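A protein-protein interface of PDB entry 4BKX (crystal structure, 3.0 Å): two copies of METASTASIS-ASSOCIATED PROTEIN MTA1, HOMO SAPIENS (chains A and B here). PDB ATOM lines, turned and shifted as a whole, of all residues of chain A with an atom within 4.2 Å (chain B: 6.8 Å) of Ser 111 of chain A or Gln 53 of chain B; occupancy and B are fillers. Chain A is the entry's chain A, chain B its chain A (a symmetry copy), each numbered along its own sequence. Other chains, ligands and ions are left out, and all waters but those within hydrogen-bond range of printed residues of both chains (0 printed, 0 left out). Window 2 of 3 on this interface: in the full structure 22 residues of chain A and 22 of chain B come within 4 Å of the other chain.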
ATOM      1  N   SER A 107      26.883  16.632  17.823  1.00  0.00           N
ATOM      2  CA  SER A 107      26.277  17.241  19.002  1.00  0.00           C
ATOM      3  C   SER A 107      25.290  16.306  19.693  1.00  0.00           C
ATOM      4  O   SER A 107      25.350  16.116  20.908  1.00  0.00           O
ATOM      5  CB  SER A 107      25.580  18.546  18.613  1.00  0.00           C
ATOM      6  OG  SER A 107      24.808  19.050  19.688  1.00  0.00           O
ATOM      7  N   LYS A 108      24.393  15.723  18.907  1.00  0.00           N
ATOM      8  CA  LYS A 108      23.364  14.823  19.414  1.00  0.00           C
ATOM      9  C   LYS A 108      23.974  13.518  19.932  1.00  0.00           C
ATOM     10  O   LYS A 108      23.565  13.006  20.979  1.00  0.00           O
ATOM     11  CB  LYS A 108      22.341  14.551  18.309  1.00  0.00           C
ATOM     12  CG  LYS A 108      20.966  14.097  18.777  1.00  0.00           C
ATOM     13  CD  LYS A 108      19.941  14.279  17.660  1.00  0.00           C
ATOM     14  CE  LYS A 108      18.935  13.133  17.603  1.00  0.00           C
ATOM     15  NZ  LYS A 108      17.973  13.131  18.743  1.00  0.00           N
ATOM     16  N   ALA A 109      24.961  13.002  19.200  1.00  0.00           N
ATOM     17  CA  ALA A 109      25.598  11.721  19.514  1.00  0.00           C
ATOM     18  C   ALA A 109      26.425  11.767  20.796  1.00  0.00           C
ATOM     19  O   ALA A 109      26.572  10.756  21.483  1.00  0.00           O
ATOM     20  CB  ALA A 109      26.451  11.250  18.346  1.00  0.00           C
ATOM     21  N   ILE A 110      26.965  12.939  21.112  1.00  0.00           N
ATOM     22  CA  ILE A 110      27.730  13.123  22.343  1.00  0.00           C
ATOM     23  C   ILE A 110      26.822  13.118  23.577  1.00  0.00           C
ATOM     24  O   ILE A 110      27.201  12.597  24.629  1.00  0.00           O
ATOM     25  CB  ILE A 110      28.647  14.364  22.257  1.00  0.00           C
ATOM     26  CG1 ILE A 110      30.041  13.921  21.813  1.00  0.00           C
ATOM     27  CG2 ILE A 110      28.757  15.080  23.595  1.00  0.00           C
ATOM     28  CD1 ILE A 110      30.641  14.758  20.700  1.00  0.00           C
ATOM     29  N   SER A 111      25.619  13.673  23.428  1.00  0.00           N
ATOM     30  CA  SER A 111      24.599  13.620  24.477  1.00  0.00           C
ATOM     31  C   SER A 111      24.187  12.183  24.785  1.00  0.00           C
ATOM     32  O   SER A 111      23.849  11.862  25.925  1.00  0.00           O
ATOM     33  CB  SER A 111      23.369  14.445  24.091  1.00  0.00           C
ATOM     34  OG  SER A 111      23.555  15.816  24.399  1.00  0.00           O
ATOM     35  N   ALA A 112      24.220  11.324  23.766  1.00  0.00           N
ATOM     36  CA  ALA A 112      23.895   9.910  23.936  1.00  0.00           C
ATOM     37  C   ALA A 112      24.956   9.189  24.762  1.00  0.00           C
ATOM     38  O   ALA A 112      24.654   8.222  25.463  1.00  0.00           O
ATOM     39  CB  ALA A 112      23.720   9.238  22.586  1.00  0.00           C
ATOM     40  N   LEU A 113      26.194   9.672  24.677  1.00  0.00           N
ATOM     41  CA  LEU A 113      27.301   9.140  25.474  1.00  0.00           C
ATOM     42  C   LEU A 113      27.214   9.538  26.948  1.00  0.00           C
ATOM     43  O   LEU A 113      27.672   8.800  27.817  1.00  0.00           O
ATOM     44  CB  LEU A 113      28.646   9.599  24.903  1.00  0.00           C
ATOM     45  CG  LEU A 113      29.116   9.041  23.563  1.00  0.00           C
ATOM     46  CD1 LEU A 113      30.351   9.800  23.113  1.00  0.00           C
ATOM     47  CD2 LEU A 113      29.409   7.553  23.667  1.00  0.00           C
ATOM     48  N   VAL A 114      26.644  10.711  27.219  1.00  0.00           N
ATOM     49  CA  VAL A 114      26.523  11.229  28.583  1.00  0.00           C
ATOM     50  C   VAL A 114      25.060  11.616  28.881  1.00  0.00           C
ATOM     51  O   VAL A 114      24.748  12.801  29.035  1.00  0.00           O
ATOM     52  CB  VAL A 114      27.472  12.432  28.822  1.00  0.00           C
ATOM     53  CG1 VAL A 114      27.570  12.753  30.301  1.00  0.00           C
ATOM     54  CG2 VAL A 114      28.865  12.154  28.280  1.00  0.00           C
ATOM     55  N   PRO A 115      24.161  10.610  28.965  1.00  0.00           N
ATOM     56  CA  PRO A 115      22.703  10.782  29.043  1.00  0.00           C
ATOM     57  C   PRO A 115      22.165  11.827  30.030  1.00  0.00           C
ATOM     58  O   PRO A 115      21.300  12.629  29.662  1.00  0.00           O
ATOM     59  CB  PRO A 115      22.219   9.388  29.438  1.00  0.00           C
ATOM     60  CG  PRO A 115      23.195   8.486  28.779  1.00  0.00           C
ATOM     61  CD  PRO A 115      24.518   9.177  28.950  1.00  0.00           C
ATOM     62  N   THR B  47      21.030  24.367  26.529  1.00  0.00           N
ATOM     63  CA  THR B  47      20.353  24.163  27.801  1.00  0.00           C
ATOM     64  C   THR B  47      21.350  23.798  28.899  1.00  0.00           C
ATOM     65  O   THR B  47      22.452  23.322  28.610  1.00  0.00           O
ATOM     66  CB  THR B  47      19.264  23.073  27.697  1.00  0.00           C
ATOM     67  OG1 THR B  47      18.688  22.855  28.991  1.00  0.00           O
ATOM     68  CG2 THR B  47      19.835  21.752  27.163  1.00  0.00           C
ATOM     69  N   ASP B  48      20.954  24.021  30.155  1.00  0.00           N
ATOM     70  CA  ASP B  48      21.754  23.628  31.323  1.00  0.00           C
ATOM     71  C   ASP B  48      22.231  22.183  31.227  1.00  0.00           C
ATOM     72  O   ASP B  48      23.326  21.853  31.685  1.00  0.00           O
ATOM     73  CB  ASP B  48      20.959  23.819  32.620  1.00  0.00           C
ATOM     74  CG  ASP B  48      20.946  25.263  33.104  1.00  0.00           C
ATOM     75  OD1 ASP B  48      21.579  26.127  32.460  1.00  0.00           O
ATOM     76  OD2 ASP B  48      20.299  25.534  34.140  1.00  0.00           O
ATOM     77  N   LYS B  49      21.402  21.333  30.625  1.00  0.00           N
ATOM     78  CA  LYS B  49      21.728  19.925  30.453  1.00  0.00           C
ATOM     79  C   LYS B  49      22.914  19.739  29.509  1.00  0.00           C
ATOM     80  O   LYS B  49      23.879  19.053  29.857  1.00  0.00           O
ATOM     81  CB  LYS B  49      20.515  19.146  29.945  1.00  0.00           C
ATOM     82  CG  LYS B  49      20.590  17.656  30.232  1.00  0.00           C
ATOM     83  CD  LYS B  49      19.489  16.894  29.519  1.00  0.00           C
ATOM     84  CE  LYS B  49      19.572  15.413  29.847  1.00  0.00           C
ATOM     85  NZ  LYS B  49      18.764  14.588  28.906  1.00  0.00           N
ATOM     86  N   GLN B  50      22.842  20.357  28.330  1.00  0.00           N
ATOM     87  CA  GLN B  50      23.897  20.241  27.321  1.00  0.00           C
ATOM     88  C   GLN B  50      25.236  20.777  27.810  1.00  0.00           C
ATOM     89  O   GLN B  50      26.278  20.175  27.564  1.00  0.00           O
ATOM     90  CB  GLN B  50      23.493  20.941  26.027  1.00  0.00           C
ATOM     91  CG  GLN B  50      22.610  20.105  25.119  1.00  0.00           C
ATOM     92  CD  GLN B  50      22.107  20.887  23.922  1.00  0.00           C
ATOM     93  OE1 GLN B  50      21.343  21.844  24.064  1.00  0.00           O
ATOM     94  NE2 GLN B  50      22.528  20.477  22.733  1.00  0.00           N
ATOM     95  N   ILE B  51      25.200  21.907  28.506  1.00  0.00           N
ATOM     96  CA  ILE B  51      26.400  22.489  29.091  1.00  0.00           C
ATOM     97  C   ILE B  51      26.964  21.555  30.161  1.00  0.00           C
ATOM     98  O   ILE B  51      28.174  21.336  30.215  1.00  0.00           O
ATOM     99  CB  ILE B  51      26.130  23.897  29.665  1.00  0.00           C
ATOM    100  CG1 ILE B  51      25.554  24.811  28.576  1.00  0.00           C
ATOM    101  CG2 ILE B  51      27.405  24.504  30.237  1.00  0.00           C
ATOM    102  CD1 ILE B  51      24.714  25.953  29.108  1.00  0.00           C
ATOM    103  N   ASP B  52      26.084  20.990  30.989  1.00  0.00           N
ATOM    104  CA  ASP B  52      26.495  20.027  32.017  1.00  0.00           C
ATOM    105  C   ASP B  52      27.145  18.792  31.397  1.00  0.00           C
ATOM    106  O   ASP B  52      28.185  18.331  31.873  1.00  0.00           O
ATOM    107  CB  ASP B  52      25.317  19.624  32.910  1.00  0.00           C
ATOM    108  CG  ASP B  52      25.097  20.593  34.071  1.00  0.00           C
ATOM    109  OD1 ASP B  52      25.785  21.633  34.141  1.00  0.00           O
ATOM    110  OD2 ASP B  52      24.230  20.310  34.925  1.00  0.00           O
ATOM    111  N   GLN B  53      26.527  18.283  30.330  1.00  0.00           N
ATOM    112  CA  GLN B  53      27.062  17.157  29.565  1.00  0.00           C
ATOM    113  C   GLN B  53      28.422  17.495  28.973  1.00  0.00           C
ATOM    114  O   GLN B  53      29.350  16.696  29.060  1.00  0.00           O
ATOM    115  CB  GLN B  53      26.101  16.749  28.448  1.00  0.00           C
ATOM    116  CG  GLN B  53      24.813  16.096  28.924  1.00  0.00           C
ATOM    117  CD  GLN B  53      23.811  15.897  27.804  1.00  0.00           C
ATOM    118  OE1 GLN B  53      23.634  16.761  26.940  1.00  0.00           O
ATOM    119  NE2 GLN B  53      23.143  14.752  27.815  1.00  0.00           N
ATOM    120  N   PHE B  54      28.537  18.680  28.382  1.00  0.00           N
ATOM    121  CA  PHE B  54      29.792  19.114  27.784  1.00  0.00           C
ATOM    122  C   PHE B  54      30.925  19.181  28.804  1.00  0.00           C
ATOM    123  O   PHE B  54      32.053  18.813  28.490  1.00  0.00           O
ATOM    124  CB  PHE B  54      29.636  20.456  27.062  1.00  0.00           C
ATOM    125  CG  PHE B  54      30.850  20.858  26.267  1.00  0.00           C
ATOM    126  CD1 PHE B  54      31.070  20.338  24.992  1.00  0.00           C
ATOM    127  CD2 PHE B  54      31.785  21.742  26.797  1.00  0.00           C
ATOM    128  CE1 PHE B  54      32.195  20.692  24.264  1.00  0.00           C
ATOM    129  CE2 PHE B  54      32.911  22.102  26.072  1.00  0.00           C
ATOM    130  CZ  PHE B  54      33.115  21.576  24.804  1.00  0.00           C
ATOM    131  N   LEU B  55      30.620  19.636  30.019  1.00  0.00           N
ATOM    132  CA  LEU B  55      31.619  19.709  31.089  1.00  0.00           C
ATOM    133  C   LEU B  55      32.075  18.326  31.558  1.00  0.00           C
ATOM    134  O   LEU B  55      33.203  18.168  32.037  1.00  0.00           O
ATOM    135  CB  LEU B  55      31.111  20.529  32.282  1.00  0.00           C
ATOM    136  CG  LEU B  55      30.813  22.027  32.133  1.00  0.00           C
ATOM    137  CD1 LEU B  55      30.735  22.682  33.506  1.00  0.00           C
ATOM    138  CD2 LEU B  55      31.835  22.752  31.270  1.00  0.00           C
ATOM    139  N   VAL B  56      31.196  17.334  31.429  1.00  0.00           N
ATOM    140  CA  VAL B  56      31.560  15.947  31.711  1.00  0.00           C
ATOM    141  C   VAL B  56      32.505  15.462  30.618  1.00  0.00           C
ATOM    142  O   VAL B  56      33.521  14.820  30.906  1.00  0.00           O
ATOM    143  CB  VAL B  56      30.329  15.014  31.796  1.00  0.00           C
ATOM    144  CG1 VAL B  56      30.752  13.590  32.118  1.00  0.00           C
ATOM    145  CG2 VAL B  56      29.350  15.504  32.849  1.00  0.00           C
ATOM    146  N   VAL B  57      32.171  15.786  29.370  1.00  0.00           N
ATOM    147  CA  VAL B  57      32.987  15.397  28.223  1.00  0.00           C
ATOM    148  C   VAL B  57      34.361  16.056  28.298  1.00  0.00           C
ATOM    149  O   VAL B  57      35.376  15.410  28.043  1.00  0.00           O
ATOM    150  CB  VAL B  57      32.305  15.743  26.883  1.00  0.00           C
ATOM    151  CG1 VAL B  57      33.161  15.281  25.708  1.00  0.00           C
ATOM    152  CG2 VAL B  57      30.932  15.097  26.802  1.00  0.00           C
ATOM    153  N   ALA B  58      34.384  17.335  28.667  1.00  0.00           N
ATOM    154  CA  ALA B  58      35.632  18.088  28.813  1.00  0.00           C
ATOM    155  C   ALA B  58      36.524  17.472  29.879  1.00  0.00           C
ATOM    156  O   ALA B  58      37.743  17.403  29.716  1.00  0.00           O
ATOM    157  CB  ALA B  58      35.341  19.541  29.142  1.00  0.00           C
ATOM    158  N   ILE B 106      28.046  22.631  19.961  1.00  0.00           N
ATOM    159  CA  ILE B 106      28.582  21.455  20.655  1.00  0.00           C
ATOM    160  C   ILE B 106      29.526  20.657  19.754  1.00  0.00           C
ATOM    161  O   ILE B 106      30.644  20.322  20.153  1.00  0.00           O
ATOM    162  CB  ILE B 106      27.443  20.545  21.179  1.00  0.00           C
ATOM    163  CG1 ILE B 106      26.579  21.280  22.218  1.00  0.00           C
ATOM    164  CG2 ILE B 106      27.983  19.238  21.743  1.00  0.00           C
ATOM    165  CD1 ILE B 106      27.274  21.622  23.524  1.00  0.00           C
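The side-chain amide oxygen (OE1) of Gln 53 of chain B lies within hydrogen-bond range of the side-chain hydroxyl (OG) of Ser 111 of chain A (2.7 Å).
O of Val 114 of chain A lies within hydrogen-bond range of NE2 of Gln 53 of chain B (2.8 Å).
The side-chain amino group of Lys 49 of chain B sits close to the backbone carbonyl oxygen of Pro 115 of chain A (3.3 Å).
O of Pro 115 of chain A lies within hydrogen-bond range of NE2 of Gln 53 of chain B, 3.4 Å away.
Of the 9 printed residues of chain A, 5 touch a printed residue of chain B.
Hydrophobic or aromatic side chains of chain A within 4 Å of the printed part of chain B: Ile 110 and Val 114.
Printed residues of chain B that touch a printed residue of chain A: Lys 49, Gln 53, Val 56, Val 57 and Ile 106.
Hydrophobic or aromatic side chains of chain B within 4 Å of the printed part of chain A: Val 56, Val 57 and Ile 106.
Among the printed residues, merely in contact across the chains: Ser 107 of chain A with Ile 106 of chain B (3.4 Å), Val 114 of chain A with Val 56 of chain B (3.8 Å), Ile 110 of chain A with Val 57 of chain B (3.9 Å) and Val 114 of chain A with Val 57 of chain B (3.9 Å).
Ser 111 of chain A touches just one residue of chain B: Gln 53.
Of the printed residues of chain B, Val 114 of chain A touches Gln 53, Val 56 and Val 57.
Printed residues of chain A within 4 Å of Lys 49 of chain B: Pro 115.
Of the printed residues of chain A, Gln 53 of chain B touches Ser 111, Val 114 and Pro 115.
Printed residues of chain A within 4 Å of Val 57 of chain B: Ile 110 (3.9 Å) and Val 114 (3.9 Å).
The nearest residue of chain B that does not touch Ser 111 of chain A is Gln 50 of chain B (4.5 Å).
The nearest printed residue of chain B that does not touch Val 114 of chain A is Asp 52 of chain B (5.8 Å).
No position is printed for both chains.
Of the 8 pairs that touch across the chains among the printed residues, none has its exchanged pair printed and touching as well.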
